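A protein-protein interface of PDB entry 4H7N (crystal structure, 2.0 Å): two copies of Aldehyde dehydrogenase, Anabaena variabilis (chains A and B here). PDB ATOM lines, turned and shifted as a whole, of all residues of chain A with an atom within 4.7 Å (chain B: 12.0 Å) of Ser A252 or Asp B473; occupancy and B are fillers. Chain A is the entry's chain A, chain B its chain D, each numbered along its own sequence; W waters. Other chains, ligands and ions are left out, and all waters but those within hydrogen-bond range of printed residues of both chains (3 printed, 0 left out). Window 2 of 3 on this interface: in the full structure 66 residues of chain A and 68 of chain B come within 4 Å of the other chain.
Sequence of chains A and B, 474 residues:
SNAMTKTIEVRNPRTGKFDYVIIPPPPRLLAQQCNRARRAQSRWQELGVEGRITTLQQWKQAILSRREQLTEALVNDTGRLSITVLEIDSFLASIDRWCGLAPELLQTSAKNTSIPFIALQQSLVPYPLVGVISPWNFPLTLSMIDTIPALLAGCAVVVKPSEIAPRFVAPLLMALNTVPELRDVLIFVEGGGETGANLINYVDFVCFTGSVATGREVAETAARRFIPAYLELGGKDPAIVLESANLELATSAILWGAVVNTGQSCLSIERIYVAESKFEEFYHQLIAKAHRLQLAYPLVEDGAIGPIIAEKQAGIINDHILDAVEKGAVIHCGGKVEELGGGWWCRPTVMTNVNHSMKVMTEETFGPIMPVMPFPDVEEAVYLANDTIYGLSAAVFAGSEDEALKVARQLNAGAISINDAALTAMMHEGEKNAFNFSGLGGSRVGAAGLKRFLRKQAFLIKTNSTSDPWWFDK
The side-chain hydroxyl (OG) of Ser A252 sits at hydrogen-bond distance from the side-chain carboxylate (OD2) of Asp B473 (2.9 Å). O of Trp B470 is in hydrogen-bond range of NE1 of Trp A256 (3.1 Å).
O of Glu A248 is in hydrogen-bond range of OG of Ser A252 (3.4 Å). The side-chain hydroxyl (OG) of Ser A252 sits at hydrogen-bond distance from the side-chain amino group (NZ) of Lys A289. NZ of Lys B462 lies within hydrogen-bond range of O of Thr B466, 2.7 Å away. OG of Ser B467 sits at hydrogen-bond distance from OD1 of Asp B473 (3.3 Å). The indole nitrogen (NE1) of Trp B470 lies close to the side-chain carboxylate (OD2) of Asp B468 (3.5 Å). The side-chain carboxylate of Asp B468 is in hydrogen-bond range of the indole nitrogen of Trp B471 (3.3 Å).
Among the printed residues, pairs that only touch across the chains: Leu A249 with Ser B465, Leu A249 with Thr B466, Leu A249 with Trp B471, Ser A252 with Trp B471, Ala A253 with Trp B471, Trp A256 with Trp B471 and Trp A256 with Phe B472.
No residue of chain B comes within 4 Å of Glu A248. No residue of chain B comes within 4 Å of Ala A250. Of chain B, only Trp B471 (3.5 Å) and Asp B473 (2.9 Å) come within 4 Å of Ser A252. Ala A253 touches just one residue of chain B: Trp B471 (3.4 Å). No residue of chain B comes within 4 Å of Ile A254. No residue of chain B comes within 4 Å of Leu A255. Of the printed residues of chain B, Trp A256 touches Trp B470 (3.1 Å), Trp B471 (3.7 Å) and Phe B472 (3.8 Å). Of the printed residues of chain A, Thr B466 touches Leu A249. Asp B468 touches none of the printed residues of chain A. Of the printed residues of chain A, Trp B471 touches Leu A249, Ser A252, Ala A253 and Trp A256. Printed residues of chain A within 4 Å of Phe B472: Trp A256 (3.8 Å). The nearest residue of chain B that does not touch Ser A252 is Ser B467 (5.5 Å).
Of the 12 printed residues of chain B, 6 touch a printed residue of chain A. Printed residues of chain B that touch a printed residue of chain A: Ser B465, Thr B466, Trp B470, Trp B471, Phe B472 and Asp B473. Hydrophobic or aromatic side chains of chain B within 4 Å of the printed part of chain A: Trp B470, Trp B471 and Phe B472. Of the 11 printed residues of chain A, 4 touch a printed residue of chain B. Printed residues of chain A that touch a printed residue of chain B: Leu A249, Ser A252, Ala A253 and Trp A256.
No position is printed for both chains.
Water W3 lies within hydrogen-bond range of the side-chain hydroxyl (OG) of Ser A252 (2.8 Å), the side-chain carboxylate (OD2) of Asp B473 (3.1 Å) and the backbone carbonyl oxygen (O) of Glu A248 (3.3 Å). Water W1 lies within hydrogen-bond range of O of Trp B470 (2.9 Å) and NE1 of Trp A256 (3.2 Å). Water W2 bridges the backbone carbonyl oxygen (O) of Ser A252 and the backbone NH (N) of Phe B472.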
ATOM      1  N   GLU A 248      -9.312 -17.745 -16.189  1.00  0.00           N
ATOM      2  CA  GLU A 248      -8.642 -17.292 -17.385  1.00  0.00           C
ATOM      3  C   GLU A 248      -7.346 -18.075 -17.626  1.00  0.00           C
ATOM      4  O   GLU A 248      -7.088 -18.536 -18.746  1.00  0.00           O
ATOM      5  CB  GLU A 248      -8.380 -15.775 -17.271  1.00  0.00           C
ATOM      6  CG  GLU A 248      -7.561 -15.214 -18.405  1.00  0.00           C
ATOM      7  CD  GLU A 248      -8.278 -15.308 -19.741  1.00  0.00           C
ATOM      8  OE1 GLU A 248      -9.490 -14.996 -19.806  1.00  0.00           O
ATOM      9  OE2 GLU A 248      -7.625 -15.671 -20.727  1.00  0.00           O
ATOM     10  N   LEU A 249      -6.526 -18.226 -16.572  1.00  0.00           N
ATOM     11  CA  LEU A 249      -5.332 -19.010 -16.658  1.00  0.00           C
ATOM     12  C   LEU A 249      -5.687 -20.492 -16.764  1.00  0.00           C
ATOM     13  O   LEU A 249      -5.083 -21.237 -17.538  1.00  0.00           O
ATOM     14  CB  LEU A 249      -4.441 -18.785 -15.410  1.00  0.00           C
ATOM     15  CG  LEU A 249      -3.853 -17.353 -15.324  1.00  0.00           C
ATOM     16  CD1 LEU A 249      -3.009 -17.208 -14.039  1.00  0.00           C
ATOM     17  CD2 LEU A 249      -3.029 -16.938 -16.555  1.00  0.00           C
ATOM     18  N   ALA A 250      -6.667 -20.933 -15.995  1.00  0.00           N
ATOM     19  CA  ALA A 250      -6.995 -22.374 -15.993  1.00  0.00           C
ATOM     20  C   ALA A 250      -7.464 -22.840 -17.380  1.00  0.00           C
ATOM     21  O   ALA A 250      -7.109 -23.934 -17.836  1.00  0.00           O
ATOM     22  CB  ALA A 250      -8.052 -22.685 -14.946  1.00  0.00           C
ATOM     23  N   THR A 251      -8.278 -22.013 -18.054  1.00  0.00           N
ATOM     24  CA  THR A 251      -8.784 -22.421 -19.361  1.00  0.00           C
ATOM     25  C   THR A 251      -7.656 -22.385 -20.397  1.00  0.00           C
ATOM     26  O   THR A 251      -7.585 -23.285 -21.230  1.00  0.00           O
ATOM     27  CB  THR A 251     -10.013 -21.613 -19.826  1.00  0.00           C
ATOM     28  OG1 THR A 251      -9.698 -20.222 -19.797  1.00  0.00           O
ATOM     29  CG2 THR A 251     -11.225 -21.905 -18.960  1.00  0.00           C
ATOM     30  N   SER A 252      -6.768 -21.390 -20.371  1.00  0.00           N
ATOM     31  CA  SER A 252      -5.647 -21.416 -21.309  1.00  0.00           C
ATOM     32  C   SER A 252      -4.697 -22.615 -21.012  1.00  0.00           C
ATOM     33  O   SER A 252      -4.206 -23.270 -21.929  1.00  0.00           O
ATOM     34  CB  SER A 252      -4.845 -20.098 -21.290  1.00  0.00           C
ATOM     35  OG  SER A 252      -5.607 -18.967 -21.722  1.00  0.00           O
ATOM     36  N   ALA A 253      -4.420 -22.887 -19.737  1.00  0.00           N
ATOM     37  CA  ALA A 253      -3.466 -23.925 -19.390  1.00  0.00           C
ATOM     38  C   ALA A 253      -4.002 -25.317 -19.777  1.00  0.00           C
ATOM     39  O   ALA A 253      -3.260 -26.142 -20.304  1.00  0.00           O
ATOM     40  CB  ALA A 253      -3.167 -23.894 -17.914  1.00  0.00           C
ATOM     41  N   ILE A 254      -5.281 -25.546 -19.484  1.00  0.00           N
ATOM     42  CA  ILE A 254      -5.914 -26.857 -19.723  1.00  0.00           C
ATOM     43  C   ILE A 254      -6.088 -27.081 -21.231  1.00  0.00           C
ATOM     44  O   ILE A 254      -5.847 -28.180 -21.737  1.00  0.00           O
ATOM     45  CB  ILE A 254      -7.223 -26.981 -18.949  1.00  0.00           C
ATOM     46  CG1 ILE A 254      -6.880 -27.178 -17.461  1.00  0.00           C
ATOM     47  CG2 ILE A 254      -8.106 -28.094 -19.503  1.00  0.00           C
ATOM     48  CD1 ILE A 254      -7.997 -26.908 -16.505  1.00  0.00           C
ATOM     49  N   LEU A 255      -6.407 -26.021 -21.966  1.00  0.00           N
ATOM     50  CA  LEU A 255      -6.482 -26.166 -23.420  1.00  0.00           C
ATOM     51  C   LEU A 255      -5.138 -26.596 -23.994  1.00  0.00           C
ATOM     52  O   LEU A 255      -5.048 -27.539 -24.805  1.00  0.00           O
ATOM     53  CB  LEU A 255      -6.983 -24.863 -24.050  1.00  0.00           C
ATOM     54  CG  LEU A 255      -6.940 -24.869 -25.570  1.00  0.00           C
ATOM     55  CD1 LEU A 255      -7.903 -25.917 -26.107  1.00  0.00           C
ATOM     56  CD2 LEU A 255      -7.186 -23.477 -26.107  1.00  0.00           C
ATOM     57  N   TRP A 256      -4.073 -25.920 -23.589  1.00  0.00           N
ATOM     58  CA  TRP A 256      -2.728 -26.239 -24.076  1.00  0.00           C
ATOM     59  C   TRP A 256      -2.341 -27.664 -23.668  1.00  0.00           C
ATOM     60  O   TRP A 256      -1.907 -28.482 -24.471  1.00  0.00           O
ATOM     61  CB  TRP A 256      -1.698 -25.212 -23.599  1.00  0.00           C
ATOM     62  CG  TRP A 256      -0.347 -25.534 -24.127  1.00  0.00           C
ATOM     63  CD1 TRP A 256       0.136 -25.261 -25.389  1.00  0.00           C
ATOM     64  CD2 TRP A 256       0.666 -26.270 -23.459  1.00  0.00           C
ATOM     65  NE1 TRP A 256       1.411 -25.763 -25.524  1.00  0.00           N
ATOM     66  CE2 TRP A 256       1.761 -26.389 -24.358  1.00  0.00           C
ATOM     67  CE3 TRP A 256       0.781 -26.799 -22.172  1.00  0.00           C
ATOM     68  CZ2 TRP A 256       2.935 -27.055 -24.017  1.00  0.00           C
ATOM     69  CZ3 TRP A 256       1.941 -27.481 -21.838  1.00  0.00           C
ATOM     70  CH2 TRP A 256       3.008 -27.609 -22.759  1.00  0.00           C
ATOM     71  N   LYS A 289     -11.811 -20.481 -26.555  1.00  0.00           N
ATOM     72  CA  LYS A 289     -10.384 -20.609 -26.814  1.00  0.00           C
ATOM     73  C   LYS A 289     -10.057 -21.777 -27.741  1.00  0.00           C
ATOM     74  O   LYS A 289      -9.185 -21.674 -28.602  1.00  0.00           O
ATOM     75  CB  LYS A 289      -9.575 -20.692 -25.472  1.00  0.00           C
ATOM     76  CG  LYS A 289      -9.708 -19.428 -24.637  1.00  0.00           C
ATOM     77  CD  LYS A 289      -9.088 -19.575 -23.254  1.00  0.00           C
ATOM     78  CE  LYS A 289      -8.950 -18.199 -22.603  1.00  0.00           C
ATOM     79  NZ  LYS A 289      -8.232 -18.290 -21.296  1.00  0.00           N
ATOM     80  N   ARG A 292     -10.723 -21.070 -31.426  1.00  0.00           N
ATOM     81  CA  ARG A 292      -9.727 -20.238 -32.131  1.00  0.00           C
ATOM     82  C   ARG A 292      -8.593 -21.051 -32.781  1.00  0.00           C
ATOM     83  O   ARG A 292      -7.977 -20.573 -33.717  1.00  0.00           O
ATOM     84  CB  ARG A 292      -9.116 -19.176 -31.217  1.00  0.00           C
ATOM     85  CG  ARG A 292     -10.072 -18.061 -30.788  1.00  0.00           C
ATOM     86  CD  ARG A 292      -9.689 -17.385 -29.466  1.00  0.00           C
ATOM     87  NE  ARG A 292      -8.599 -16.408 -29.587  1.00  0.00           N
ATOM     88  CZ  ARG A 292      -7.294 -16.634 -29.363  1.00  0.00           C
ATOM     89  NH1 ARG A 292      -6.843 -17.836 -29.000  1.00  0.00           N
ATOM     90  NH2 ARG A 292      -6.420 -15.635 -29.500  1.00  0.00           N
ATOM     91  N   PHE B 117       9.126 -18.367 -12.790  1.00  0.00           N
ATOM     92  CA  PHE B 117       7.777 -18.414 -12.262  1.00  0.00           C
ATOM     93  C   PHE B 117       7.300 -19.844 -11.939  1.00  0.00           C
ATOM     94  O   PHE B 117       6.104 -20.038 -11.663  1.00  0.00           O
ATOM     95  CB  PHE B 117       6.794 -17.752 -13.243  1.00  0.00           C
ATOM     96  CG  PHE B 117       6.837 -18.299 -14.629  1.00  0.00           C
ATOM     97  CD1 PHE B 117       6.045 -19.382 -14.982  1.00  0.00           C
ATOM     98  CD2 PHE B 117       7.632 -17.678 -15.634  1.00  0.00           C
ATOM     99  CE1 PHE B 117       6.068 -19.883 -16.268  1.00  0.00           C
ATOM    100  CE2 PHE B 117       7.640 -18.172 -16.923  1.00  0.00           C
ATOM    101  CZ  PHE B 117       6.852 -19.296 -17.234  1.00  0.00           C
ATOM    102  N   LYS B 462       3.105 -22.860 -10.527  1.00  0.00           N
ATOM    103  CA  LYS B 462       3.114 -21.543 -11.163  1.00  0.00           C
ATOM    104  C   LYS B 462       2.831 -20.437 -10.153  1.00  0.00           C
ATOM    105  O   LYS B 462       1.783 -20.411  -9.499  1.00  0.00           O
ATOM    106  CB  LYS B 462       2.102 -21.469 -12.305  1.00  0.00           C
ATOM    107  CG  LYS B 462       2.078 -20.129 -13.001  1.00  0.00           C
ATOM    108  CD  LYS B 462       1.006 -20.125 -14.076  1.00  0.00           C
ATOM    109  CE  LYS B 462       0.878 -18.780 -14.776  1.00  0.00           C
ATOM    110  NZ  LYS B 462       2.056 -18.453 -15.640  1.00  0.00           N
ATOM    111  N   ASN B 464       3.179 -16.962 -10.796  1.00  0.00           N
ATOM    112  CA  ASN B 464       2.836 -15.640 -11.309  1.00  0.00           C
ATOM    113  C   ASN B 464       1.447 -15.657 -11.969  1.00  0.00           C
ATOM    114  O   ASN B 464       0.785 -16.685 -11.977  1.00  0.00           O
ATOM    115  CB  ASN B 464       3.896 -15.172 -12.315  1.00  0.00           C
ATOM    116  CG  ASN B 464       3.911 -16.033 -13.572  1.00  0.00           C
ATOM    117  OD1 ASN B 464       3.421 -17.181 -13.579  1.00  0.00           O
ATOM    118  ND2 ASN B 464       4.530 -15.522 -14.612  1.00  0.00           N
ATOM    119  N   SER B 465       1.028 -14.555 -12.578  1.00  0.00           N
ATOM    120  CA  SER B 465      -0.330 -14.522 -13.178  1.00  0.00           C
ATOM    121  C   SER B 465      -0.400 -14.181 -14.653  1.00  0.00           C
ATOM    122  O   SER B 465      -1.473 -13.844 -15.126  1.00  0.00           O
ATOM    123  CB  SER B 465      -1.198 -13.503 -12.421  1.00  0.00           C
ATOM    124  OG  SER B 465      -1.470 -13.943 -11.088  1.00  0.00           O
ATOM    125  N   THR B 466       0.721 -14.207 -15.375  1.00  0.00           N
ATOM    126  CA  THR B 466       0.671 -14.019 -16.827  1.00  0.00           C
ATOM    127  C   THR B 466       0.634 -15.366 -17.559  1.00  0.00           C
ATOM    128  O   THR B 466       0.913 -16.433 -16.960  1.00  0.00           O
ATOM    129  CB  THR B 466       1.841 -13.142 -17.318  1.00  0.00           C
ATOM    130  OG1 THR B 466       3.087 -13.764 -16.978  1.00  0.00           O
ATOM    131  CG2 THR B 466       1.786 -11.795 -16.676  1.00  0.00           C
ATOM    132  N   SER B 467       0.255 -15.341 -18.844  1.00  0.00           N
ATOM    133  CA  SER B 467       0.234 -16.578 -19.660  1.00  0.00           C
ATOM    134  C   SER B 467       1.604 -17.229 -19.691  1.00  0.00           C
ATOM    135  O   SER B 467       2.596 -16.544 -19.697  1.00  0.00           O
ATOM    136  CB  SER B 467      -0.155 -16.293 -21.107  1.00  0.00           C
ATOM    137  OG  SER B 467      -1.347 -15.573 -21.180  1.00  0.00           O
ATOM    138  N   ASP B 468       1.674 -18.552 -19.683  1.00  0.00           N
ATOM    139  CA  ASP B 468       2.925 -19.219 -19.967  1.00  0.00           C
ATOM    140  C   ASP B 468       3.281 -18.928 -21.436  1.00  0.00           C
ATOM    141  O   ASP B 468       2.397 -18.858 -22.281  1.00  0.00           O
ATOM    142  CB  ASP B 468       2.780 -20.749 -19.765  1.00  0.00           C
ATOM    143  CG  ASP B 468       2.672 -21.166 -18.294  1.00  0.00           C
ATOM    144  OD1 ASP B 468       2.892 -20.283 -17.413  1.00  0.00           O
ATOM    145  OD2 ASP B 468       2.463 -22.421 -18.048  1.00  0.00           O
ATOM    146  N   PRO B 469       4.572 -18.763 -21.747  1.00  0.00           N
ATOM    147  CA  PRO B 469       4.960 -18.393 -23.113  1.00  0.00           C
ATOM    148  C   PRO B 469       4.648 -19.450 -24.172  1.00  0.00           C
ATOM    149  O   PRO B 469       4.504 -19.097 -25.312  1.00  0.00           O
ATOM    150  CB  PRO B 469       6.473 -18.178 -23.029  1.00  0.00           C
ATOM    151  CG  PRO B 469       6.894 -18.521 -21.665  1.00  0.00           C
ATOM    152  CD  PRO B 469       5.670 -18.591 -20.783  1.00  0.00           C
ATOM    153  N   TRP B 470       4.514 -20.717 -23.764  1.00  0.00           N
ATOM    154  CA  TRP B 470       4.196 -21.812 -24.677  1.00  0.00           C
ATOM    155  C   TRP B 470       2.678 -22.053 -24.921  1.00  0.00           C
ATOM    156  O   TRP B 470       2.319 -22.841 -25.796  1.00  0.00           O
ATOM    157  CB  TRP B 470       4.850 -23.107 -24.165  1.00  0.00           C
ATOM    158  CG  TRP B 470       4.578 -23.393 -22.716  1.00  0.00           C
ATOM    159  CD1 TRP B 470       3.506 -24.005 -22.210  1.00  0.00           C
ATOM    160  CD2 TRP B 470       5.400 -23.018 -21.594  1.00  0.00           C
ATOM    161  NE1 TRP B 470       3.615 -24.119 -20.835  1.00  0.00           N
ATOM    162  CE2 TRP B 470       4.764 -23.488 -20.437  1.00  0.00           C
ATOM    163  CE3 TRP B 470       6.625 -22.357 -21.469  1.00  0.00           C
ATOM    164  CZ2 TRP B 470       5.295 -23.298 -19.150  1.00  0.00           C
ATOM    165  CZ3 TRP B 470       7.178 -22.186 -20.185  1.00  0.00           C
ATOM    166  CH2 TRP B 470       6.495 -22.665 -19.037  1.00  0.00           C
ATOM    167  N   TRP B 471       1.789 -21.385 -24.177  1.00  0.00           N
ATOM    168  CA  TRP B 471       0.363 -21.552 -24.423  1.00  0.00           C
ATOM    169  C   TRP B 471       0.006 -20.995 -25.801  1.00  0.00           C
ATOM    170  O   TRP B 471       0.798 -20.303 -26.455  1.00  0.00           O
ATOM    171  CB  TRP B 471      -0.507 -20.862 -23.351  1.00  0.00           C
ATOM    172  CG  TRP B 471      -0.380 -21.434 -21.989  1.00  0.00           C
ATOM    173  CD1 TRP B 471       0.150 -22.641 -21.658  1.00  0.00           C
ATOM    174  CD2 TRP B 471      -0.867 -20.859 -20.759  1.00  0.00           C
ATOM    175  NE1 TRP B 471       0.079 -22.832 -20.291  1.00  0.00           N
ATOM    176  CE2 TRP B 471      -0.544 -21.753 -19.724  1.00  0.00           C
ATOM    177  CE3 TRP B 471      -1.509 -19.660 -20.438  1.00  0.00           C
ATOM    178  CZ2 TRP B 471      -0.838 -21.489 -18.396  1.00  0.00           C
ATOM    179  CZ3 TRP B 471      -1.823 -19.402 -19.128  1.00  0.00           C
ATOM    180  CH2 TRP B 471      -1.479 -20.294 -18.119  1.00  0.00           C
ATOM    181  N   PHE B 472      -1.203 -21.280 -26.233  1.00  0.00           N
ATOM    182  CA  PHE B 472      -1.618 -20.853 -27.590  1.00  0.00           C
ATOM    183  C   PHE B 472      -1.977 -19.373 -27.660  1.00  0.00           C
ATOM    184  O   PHE B 472      -1.796 -18.764 -28.690  1.00  0.00           O
ATOM    185  CB  PHE B 472      -2.784 -21.707 -28.112  1.00  0.00           C
ATOM    186  CG  PHE B 472      -2.424 -23.163 -28.333  1.00  0.00           C
ATOM    187  CD1 PHE B 472      -1.466 -23.527 -29.267  1.00  0.00           C
ATOM    188  CD2 PHE B 472      -3.057 -24.153 -27.639  1.00  0.00           C
ATOM    189  CE1 PHE B 472      -1.129 -24.865 -29.491  1.00  0.00           C
ATOM    190  CE2 PHE B 472      -2.742 -25.485 -27.846  1.00  0.00           C
ATOM    191  CZ  PHE B 472      -1.770 -25.850 -28.778  1.00  0.00           C
ATOM    192  N   ASP B 473      -2.483 -18.802 -26.577  1.00  0.00           N
ATOM    193  CA  ASP B 473      -2.999 -17.424 -26.626  1.00  0.00           C
ATOM    194  C   ASP B 473      -1.886 -16.395 -26.918  1.00  0.00           C
ATOM    195  O   ASP B 473      -2.142 -15.408 -27.580  1.00  0.00           O
ATOM    196  CB  ASP B 473      -3.785 -17.069 -25.336  1.00  0.00           C
ATOM    197  CG  ASP B 473      -2.946 -17.219 -24.044  1.00  0.00           C
ATOM    198  OD1 ASP B 473      -1.699 -17.102 -24.131  1.00  0.00           O
ATOM    199  OD2 ASP B 473      -3.539 -17.437 -22.953  1.00  0.00           O
HETATM  200  O   HOH W   1       3.550 -24.705 -27.593  1.00  0.00           O
HETATM  201  O   HOH W   2      -3.536 -22.203 -24.522  1.00  0.00           O
HETATM  202  O   HOH W   3      -4.415 -17.035 -20.024  1.00  0.00           O
